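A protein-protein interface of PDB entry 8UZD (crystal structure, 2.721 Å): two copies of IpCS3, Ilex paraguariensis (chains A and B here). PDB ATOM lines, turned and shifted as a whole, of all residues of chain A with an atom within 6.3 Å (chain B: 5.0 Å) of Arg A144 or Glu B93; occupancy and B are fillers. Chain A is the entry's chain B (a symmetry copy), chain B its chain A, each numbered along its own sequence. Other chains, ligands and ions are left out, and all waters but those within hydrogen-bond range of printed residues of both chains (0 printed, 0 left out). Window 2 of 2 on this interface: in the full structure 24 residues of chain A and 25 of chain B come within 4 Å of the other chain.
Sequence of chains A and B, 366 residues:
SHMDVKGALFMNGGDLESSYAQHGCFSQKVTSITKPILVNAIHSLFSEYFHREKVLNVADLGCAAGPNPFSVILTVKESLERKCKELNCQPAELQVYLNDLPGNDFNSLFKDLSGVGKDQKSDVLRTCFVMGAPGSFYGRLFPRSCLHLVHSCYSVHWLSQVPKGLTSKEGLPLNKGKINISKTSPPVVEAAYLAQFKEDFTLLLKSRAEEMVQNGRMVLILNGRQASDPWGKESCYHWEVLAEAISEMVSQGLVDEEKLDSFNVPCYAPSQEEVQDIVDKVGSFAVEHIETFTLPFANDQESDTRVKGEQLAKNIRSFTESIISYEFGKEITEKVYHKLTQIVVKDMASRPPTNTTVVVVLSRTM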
ATOM      1  N   ARG A 140     -29.679  16.983  10.994  1.00  0.00           N
ATOM      2  CA  ARG A 140     -29.478  18.132  11.859  1.00  0.00           C
ATOM      3  C   ARG A 140     -29.957  19.399  11.144  1.00  0.00           C
ATOM      4  O   ARG A 140     -29.843  19.494   9.917  1.00  0.00           O
ATOM      5  CB  ARG A 140     -28.017  18.164  12.306  1.00  0.00           C
ATOM      6  CG  ARG A 140     -27.660  17.040  13.269  1.00  0.00           C
ATOM      7  CD  ARG A 140     -28.272  17.270  14.638  1.00  0.00           C
ATOM      8  NE  ARG A 140     -27.944  18.630  15.034  1.00  0.00           N
ATOM      9  CZ  ARG A 140     -26.823  18.978  15.651  1.00  0.00           C
ATOM     10  NH1 ARG A 140     -25.946  18.050  16.001  1.00  0.00           N
ATOM     11  NH2 ARG A 140     -26.594  20.243  15.943  1.00  0.00           N
ATOM     12  N   PHE A 142     -30.249  22.576  13.402  1.00  0.00           N
ATOM     13  CA  PHE A 142     -30.065  23.639  14.378  1.00  0.00           C
ATOM     14  C   PHE A 142     -28.894  23.323  15.303  1.00  0.00           C
ATOM     15  O   PHE A 142     -28.552  22.164  15.489  1.00  0.00           O
ATOM     16  CB  PHE A 142     -31.317  23.775  15.250  1.00  0.00           C
ATOM     17  CG  PHE A 142     -32.592  23.944  14.474  1.00  0.00           C
ATOM     18  CD1 PHE A 142     -32.869  25.137  13.813  1.00  0.00           C
ATOM     19  CD2 PHE A 142     -33.503  22.901  14.387  1.00  0.00           C
ATOM     20  CE1 PHE A 142     -34.030  25.274  13.072  1.00  0.00           C
ATOM     21  CE2 PHE A 142     -34.671  23.047  13.651  1.00  0.00           C
ATOM     22  CZ  PHE A 142     -34.933  24.233  12.997  1.00  0.00           C
ATOM     23  N   PRO A 143     -28.273  24.344  15.940  1.00  0.00           N
ATOM     24  CA  PRO A 143     -27.209  24.124  16.918  1.00  0.00           C
ATOM     25  C   PRO A 143     -27.624  23.141  18.015  1.00  0.00           C
ATOM     26  O   PRO A 143     -28.815  22.961  18.272  1.00  0.00           O
ATOM     27  CB  PRO A 143     -27.034  25.497  17.586  1.00  0.00           C
ATOM     28  CG  PRO A 143     -27.550  26.504  16.581  1.00  0.00           C
ATOM     29  CD  PRO A 143     -28.575  25.770  15.745  1.00  0.00           C
ATOM     30  N   ARG A 144     -26.613  22.543  18.662  1.00  0.00           N
ATOM     31  CA  ARG A 144     -26.774  21.606  19.764  1.00  0.00           C
ATOM     32  C   ARG A 144     -27.456  22.290  20.943  1.00  0.00           C
ATOM     33  O   ARG A 144     -27.105  23.413  21.306  1.00  0.00           O
ATOM     34  CB  ARG A 144     -25.416  21.068  20.219  1.00  0.00           C
ATOM     35  CG  ARG A 144     -24.795  20.054  19.274  1.00  0.00           C
ATOM     36  CD  ARG A 144     -23.616  19.331  19.902  1.00  0.00           C
ATOM     37  NE  ARG A 144     -23.271  18.214  19.028  1.00  0.00           N
ATOM     38  CZ  ARG A 144     -22.431  18.281  17.996  1.00  0.00           C
ATOM     39  NH1 ARG A 144     -21.822  19.418  17.709  1.00  0.00           N
ATOM     40  NH2 ARG A 144     -22.208  17.210  17.252  1.00  0.00           N
ATOM     41  N   SER A 145     -28.441  21.571  21.508  1.00  0.00           N
ATOM     42  CA  SER A 145     -29.187  21.904  22.715  1.00  0.00           C
ATOM     43  C   SER A 145     -29.434  23.405  22.879  1.00  0.00           C
ATOM     44  O   SER A 145     -28.899  24.035  23.791  1.00  0.00           O
ATOM     45  CB  SER A 145     -28.552  21.285  23.925  1.00  0.00           C
ATOM     46  OG  SER A 145     -27.172  21.573  23.946  1.00  0.00           O
ATOM     47  N   CYS A 146     -30.302  23.943  22.010  1.00  0.00           N
ATOM     48  CA  CYS A 146     -30.718  25.338  22.069  1.00  0.00           C
ATOM     49  C   CYS A 146     -32.240  25.480  21.970  1.00  0.00           C
ATOM     50  O   CYS A 146     -32.775  26.534  22.317  1.00  0.00           O
ATOM     51  CB  CYS A 146     -30.054  26.158  20.971  1.00  0.00           C
ATOM     52  SG  CYS A 146     -30.582  25.653  19.315  1.00  0.00           S
ATOM     53  N   LEU A 147     -32.933  24.433  21.503  1.00  0.00           N
ATOM     54  CA  LEU A 147     -34.376  24.519  21.323  1.00  0.00           C
ATOM     55  C   LEU A 147     -35.111  24.214  22.633  1.00  0.00           C
ATOM     56  O   LEU A 147     -34.823  23.215  23.292  1.00  0.00           O
ATOM     57  CB  LEU A 147     -34.811  23.541  20.229  1.00  0.00           C
ATOM     58  CG  LEU A 147     -34.222  23.754  18.840  1.00  0.00           C
ATOM     59  CD1 LEU A 147     -34.786  22.705  17.892  1.00  0.00           C
ATOM     60  CD2 LEU A 147     -34.515  25.158  18.328  1.00  0.00           C
ATOM     61  N   GLU A 210     -30.596  15.962  19.880  1.00  0.00           N
ATOM     62  CA  GLU A 210     -29.308  16.652  19.928  1.00  0.00           C
ATOM     63  C   GLU A 210     -29.498  18.166  20.036  1.00  0.00           C
ATOM     64  O   GLU A 210     -28.616  18.858  20.530  1.00  0.00           O
ATOM     65  CB  GLU A 210     -28.454  16.327  18.693  1.00  0.00           C
ATOM     66  CG  GLU A 210     -27.600  15.077  18.826  1.00  0.00           C
ATOM     67  CD  GLU A 210     -27.030  14.550  17.512  1.00  0.00           C
ATOM     68  OE1 GLU A 210     -27.381  13.413  17.122  1.00  0.00           O
ATOM     69  OE2 GLU A 210     -26.222  15.264  16.880  1.00  0.00           O
ATOM     70  N   GLU A 211     -30.647  18.667  19.560  1.00  0.00           N
ATOM     71  CA  GLU A 211     -30.874  20.093  19.367  1.00  0.00           C
ATOM     72  C   GLU A 211     -31.682  20.715  20.511  1.00  0.00           C
ATOM     73  O   GLU A 211     -31.797  21.939  20.582  1.00  0.00           O
ATOM     74  CB  GLU A 211     -31.530  20.333  18.000  1.00  0.00           C
ATOM     75  CG  GLU A 211     -30.621  20.000  16.831  1.00  0.00           C
ATOM     76  CD  GLU A 211     -31.320  19.927  15.488  1.00  0.00           C
ATOM     77  OE1 GLU A 211     -32.570  19.994  15.468  1.00  0.00           O
ATOM     78  OE2 GLU A 211     -30.610  19.798  14.458  1.00  0.00           O
ATOM     79  N   MET A 212     -32.233  19.888  21.410  1.00  0.00           N
ATOM     80  CA  MET A 212     -33.139  20.390  22.436  1.00  0.00           C
ATOM     81  C   MET A 212     -32.414  20.529  23.772  1.00  0.00           C
ATOM     82  O   MET A 212     -31.600  19.680  24.126  1.00  0.00           O
ATOM     83  CB  MET A 212     -34.328  19.441  22.616  1.00  0.00           C
ATOM     84  CG  MET A 212     -35.355  19.546  21.499  1.00  0.00           C
ATOM     85  SD  MET A 212     -36.571  18.197  21.522  1.00  0.00           S
ATOM     86  CE  MET A 212     -37.500  18.605  23.001  1.00  0.00           C
ATOM     87  N   LYS B  54     -19.678  26.410  21.422  1.00  0.00           N
ATOM     88  CA  LYS B  54     -20.463  25.326  20.853  1.00  0.00           C
ATOM     89  C   LYS B  54     -20.952  25.683  19.451  1.00  0.00           C
ATOM     90  O   LYS B  54     -21.050  24.821  18.581  1.00  0.00           O
ATOM     91  CB  LYS B  54     -21.623  24.991  21.799  1.00  0.00           C
ATOM     92  CG  LYS B  54     -21.183  24.667  23.224  1.00  0.00           C
ATOM     93  CD  LYS B  54     -22.188  24.997  24.312  1.00  0.00           C
ATOM     94  CE  LYS B  54     -21.536  25.025  25.677  1.00  0.00           C
ATOM     95  NZ  LYS B  54     -22.511  24.674  26.738  1.00  0.00           N
ATOM     96  N   VAL B  55     -21.278  26.962  19.239  1.00  0.00           N
ATOM     97  CA  VAL B  55     -21.716  27.422  17.932  1.00  0.00           C
ATOM     98  C   VAL B  55     -21.111  28.801  17.659  1.00  0.00           C
ATOM     99  O   VAL B  55     -20.972  29.610  18.569  1.00  0.00           O
ATOM    100  CB  VAL B  55     -23.257  27.400  17.817  1.00  0.00           C
ATOM    101  CG1 VAL B  55     -23.936  28.272  18.860  1.00  0.00           C
ATOM    102  CG2 VAL B  55     -23.767  27.736  16.419  1.00  0.00           C
ATOM    103  N   LEU B  56     -20.739  29.046  16.397  1.00  0.00           N
ATOM    104  CA  LEU B  56     -20.335  30.367  15.942  1.00  0.00           C
ATOM    105  C   LEU B  56     -21.462  30.951  15.087  1.00  0.00           C
ATOM    106  O   LEU B  56     -21.872  30.338  14.102  1.00  0.00           O
ATOM    107  CB  LEU B  56     -19.035  30.233  15.143  1.00  0.00           C
ATOM    108  CG  LEU B  56     -18.299  31.544  14.864  1.00  0.00           C
ATOM    109  CD1 LEU B  56     -17.285  31.843  15.956  1.00  0.00           C
ATOM    110  CD2 LEU B  56     -17.627  31.521  13.501  1.00  0.00           C
ATOM    111  N   LEU B  80     -12.792  28.513   9.374  1.00  0.00           N
ATOM    112  CA  LEU B  80     -13.101  27.862  10.639  1.00  0.00           C
ATOM    113  C   LEU B  80     -12.574  26.424  10.633  1.00  0.00           C
ATOM    114  O   LEU B  80     -12.018  25.967  11.624  1.00  0.00           O
ATOM    115  CB  LEU B  80     -14.612  27.942  10.908  1.00  0.00           C
ATOM    116  CG  LEU B  80     -15.101  27.324  12.220  1.00  0.00           C
ATOM    117  CD1 LEU B  80     -14.625  28.113  13.436  1.00  0.00           C
ATOM    118  CD2 LEU B  80     -16.613  27.199  12.226  1.00  0.00           C
ATOM    119  N   PRO B  91     -14.443  21.312  16.093  1.00  0.00           N
ATOM    120  CA  PRO B  91     -14.915  22.517  15.419  1.00  0.00           C
ATOM    121  C   PRO B  91     -16.274  22.897  16.012  1.00  0.00           C
ATOM    122  O   PRO B  91     -17.115  22.031  16.256  1.00  0.00           O
ATOM    123  CB  PRO B  91     -14.966  22.125  13.930  1.00  0.00           C
ATOM    124  CG  PRO B  91     -15.049  20.597  13.917  1.00  0.00           C
ATOM    125  CD  PRO B  91     -14.591  20.095  15.276  1.00  0.00           C
ATOM    126  N   ALA B  92     -16.449  24.192  16.303  1.00  0.00           N
ATOM    127  CA  ALA B  92     -17.756  24.731  16.638  1.00  0.00           C
ATOM    128  C   ALA B  92     -18.678  24.513  15.449  1.00  0.00           C
ATOM    129  O   ALA B  92     -18.217  24.392  14.317  1.00  0.00           O
ATOM    130  CB  ALA B  92     -17.643  26.197  16.957  1.00  0.00           C
ATOM    131  N   GLU B  93     -19.983  24.434  15.722  1.00  0.00           N
ATOM    132  CA  GLU B  93     -20.948  24.421  14.641  1.00  0.00           C
ATOM    133  C   GLU B  93     -21.101  25.848  14.127  1.00  0.00           C
ATOM    134  O   GLU B  93     -20.770  26.804  14.826  1.00  0.00           O
ATOM    135  CB  GLU B  93     -22.265  23.798  15.094  1.00  0.00           C
ATOM    136  CG  GLU B  93     -22.157  22.290  15.183  1.00  0.00           C
ATOM    137  CD  GLU B  93     -23.321  21.594  15.852  1.00  0.00           C
ATOM    138  OE1 GLU B  93     -23.554  20.406  15.526  1.00  0.00           O
ATOM    139  OE2 GLU B  93     -23.983  22.240  16.695  1.00  0.00           O
ATOM    140  N   LEU B  94     -21.598  25.977  12.895  1.00  0.00           N
ATOM    141  CA  LEU B  94     -21.724  27.292  12.300  1.00  0.00           C
ATOM    142  C   LEU B  94     -23.197  27.595  12.047  1.00  0.00           C
ATOM    143  O   LEU B  94     -23.906  26.791  11.439  1.00  0.00           O
ATOM    144  CB  LEU B  94     -20.903  27.315  11.009  1.00  0.00           C
ATOM    145  CG  LEU B  94     -21.005  28.602  10.191  1.00  0.00           C
ATOM    146  CD1 LEU B  94     -20.321  29.765  10.898  1.00  0.00           C
ATOM    147  CD2 LEU B  94     -20.480  28.400   8.775  1.00  0.00           C
ATOM    148  N   GLN B  95     -23.656  28.754  12.531  1.00  0.00           N
ATOM    149  CA  GLN B  95     -24.991  29.207  12.173  1.00  0.00           C
ATOM    150  C   GLN B  95     -24.875  30.540  11.442  1.00  0.00           C
ATOM    151  O   GLN B  95     -24.302  31.493  11.980  1.00  0.00           O
ATOM    152  CB  GLN B  95     -25.905  29.292  13.400  1.00  0.00           C
ATOM    153  CG  GLN B  95     -27.283  29.858  13.082  1.00  0.00           C
ATOM    154  CD  GLN B  95     -28.285  29.778  14.205  1.00  0.00           C
ATOM    155  OE1 GLN B  95     -29.441  29.404  13.994  1.00  0.00           O
ATOM    156  NE2 GLN B  95     -27.857  30.148  15.404  1.00  0.00           N
ATOM    157  N   THR B 127     -22.943  20.435   9.643  1.00  0.00           N
ATOM    158  CA  THR B 127     -22.723  21.214  10.860  1.00  0.00           C
ATOM    159  C   THR B 127     -22.726  22.711  10.532  1.00  0.00           C
ATOM    160  O   THR B 127     -22.144  23.536  11.249  1.00  0.00           O
ATOM    161  CB  THR B 127     -21.578  20.684  11.738  1.00  0.00           C
ATOM    162  OG1 THR B 127     -20.415  20.487  10.935  1.00  0.00           O
ATOM    163  CG2 THR B 127     -21.932  19.396  12.449  1.00  0.00           C
ATOM    164  N   PHE B 129     -25.587  25.582   9.441  1.00  0.00           N
ATOM    165  CA  PHE B 129     -27.015  25.823   9.532  1.00  0.00           C
ATOM    166  C   PHE B 129     -27.326  27.233   9.044  1.00  0.00           C
ATOM    167  O   PHE B 129     -27.019  28.206   9.735  1.00  0.00           O
ATOM    168  CB  PHE B 129     -27.481  25.601  10.972  1.00  0.00           C
ATOM    169  CG  PHE B 129     -27.021  24.296  11.569  1.00  0.00           C
ATOM    170  CD1 PHE B 129     -27.310  23.087  10.939  1.00  0.00           C
ATOM    171  CD2 PHE B 129     -26.292  24.271  12.749  1.00  0.00           C
ATOM    172  CE1 PHE B 129     -26.881  21.878  11.480  1.00  0.00           C
ATOM    173  CE2 PHE B 129     -25.867  23.065  13.289  1.00  0.00           C
ATOM    174  CZ  PHE B 129     -26.174  21.872  12.665  1.00  0.00           C
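The backbone carbonyl oxygen (O) of Lys B54 sits at hydrogen-bond distance from the backbone NH (N) of Glu B93. The backbone NH (N) of Phe A142 is in hydrogen-bond range of the side-chain carboxylate (OE2) of Glu A211, at 3.0 Å. The backbone NH (N) of Phe B129 is in hydrogen-bond range of the backbone carbonyl oxygen (O) of Leu B94 (2.9 Å). The side-chain sulfur (SG) of Cys A146 is in hydrogen-bond range of the backbone carbonyl oxygen (O) of Pro A143. The side-chain carboxylate (OE2) of Glu A211 is in salt-bridge range of the guanidinium group (NE) of Arg A140 (3.0 Å). The backbone NH of Leu B56 is in hydrogen-bond range of the backbone carbonyl oxygen of Glu B93, 2.7 Å away.
Among the printed residues, merely in contact across the chains: Phe A142 with Phe B129, Arg A140 with Phe B129, Pro A143 with Glu B93, Pro A143 with Phe B129, Pro A143 with Gln B95 and Pro A143 with Val B55.
The side-chain carboxylate (OE1) of Glu B93 is in salt-bridge range of the guanidinium group (NH1) of Arg A144 (3.0 Å). The side-chain carboxylate (OE1) of Glu B93 lies within salt-bridge range of the guanidinium group (NH2) of Arg A140 (3.1 Å).
No position is printed for both chains. Of the 8 pairs that touch across the chains among the printed residues, none has its exchanged pair printed and touching as well.
Of chain B, only Glu B93 (3.0 Å) comes within 4 Å of Arg A144. Of chain A, only Arg A140 (3.1 Å), Pro A143 (3.7 Å) and Arg A144 (3.0 Å) come within 4 Å of Glu B93. Of the printed residues of chain B, Phe A142 touches Phe B129 (3.6 Å). Of the printed residues of chain A, Val B55 touches Pro A143. Printed residues of chain A within 4 Å of Phe B129: Arg A140 (3.7 Å), Phe A142 (3.6 Å) and Pro A143 (3.8 Å).
Of the 10 printed residues of chain A, 4 touch a printed residue of chain B. Printed residues of chain A that touch a printed residue of chain B: Arg A140, Phe A142, Pro A143 and Arg A144. Hydrophobic or aromatic side chains of chain A within 4 Å of the printed part of chain B: Pro A143. Along chain A the printed residues that touch a printed residue of chain B span positions 140 to 144. Of the 11 printed residues of chain B, 4 touch a printed residue of chain A. Hydrophobic or aromatic side chains of chain B within 4 Å of the printed part of chain A: Val B55 and Phe B129.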
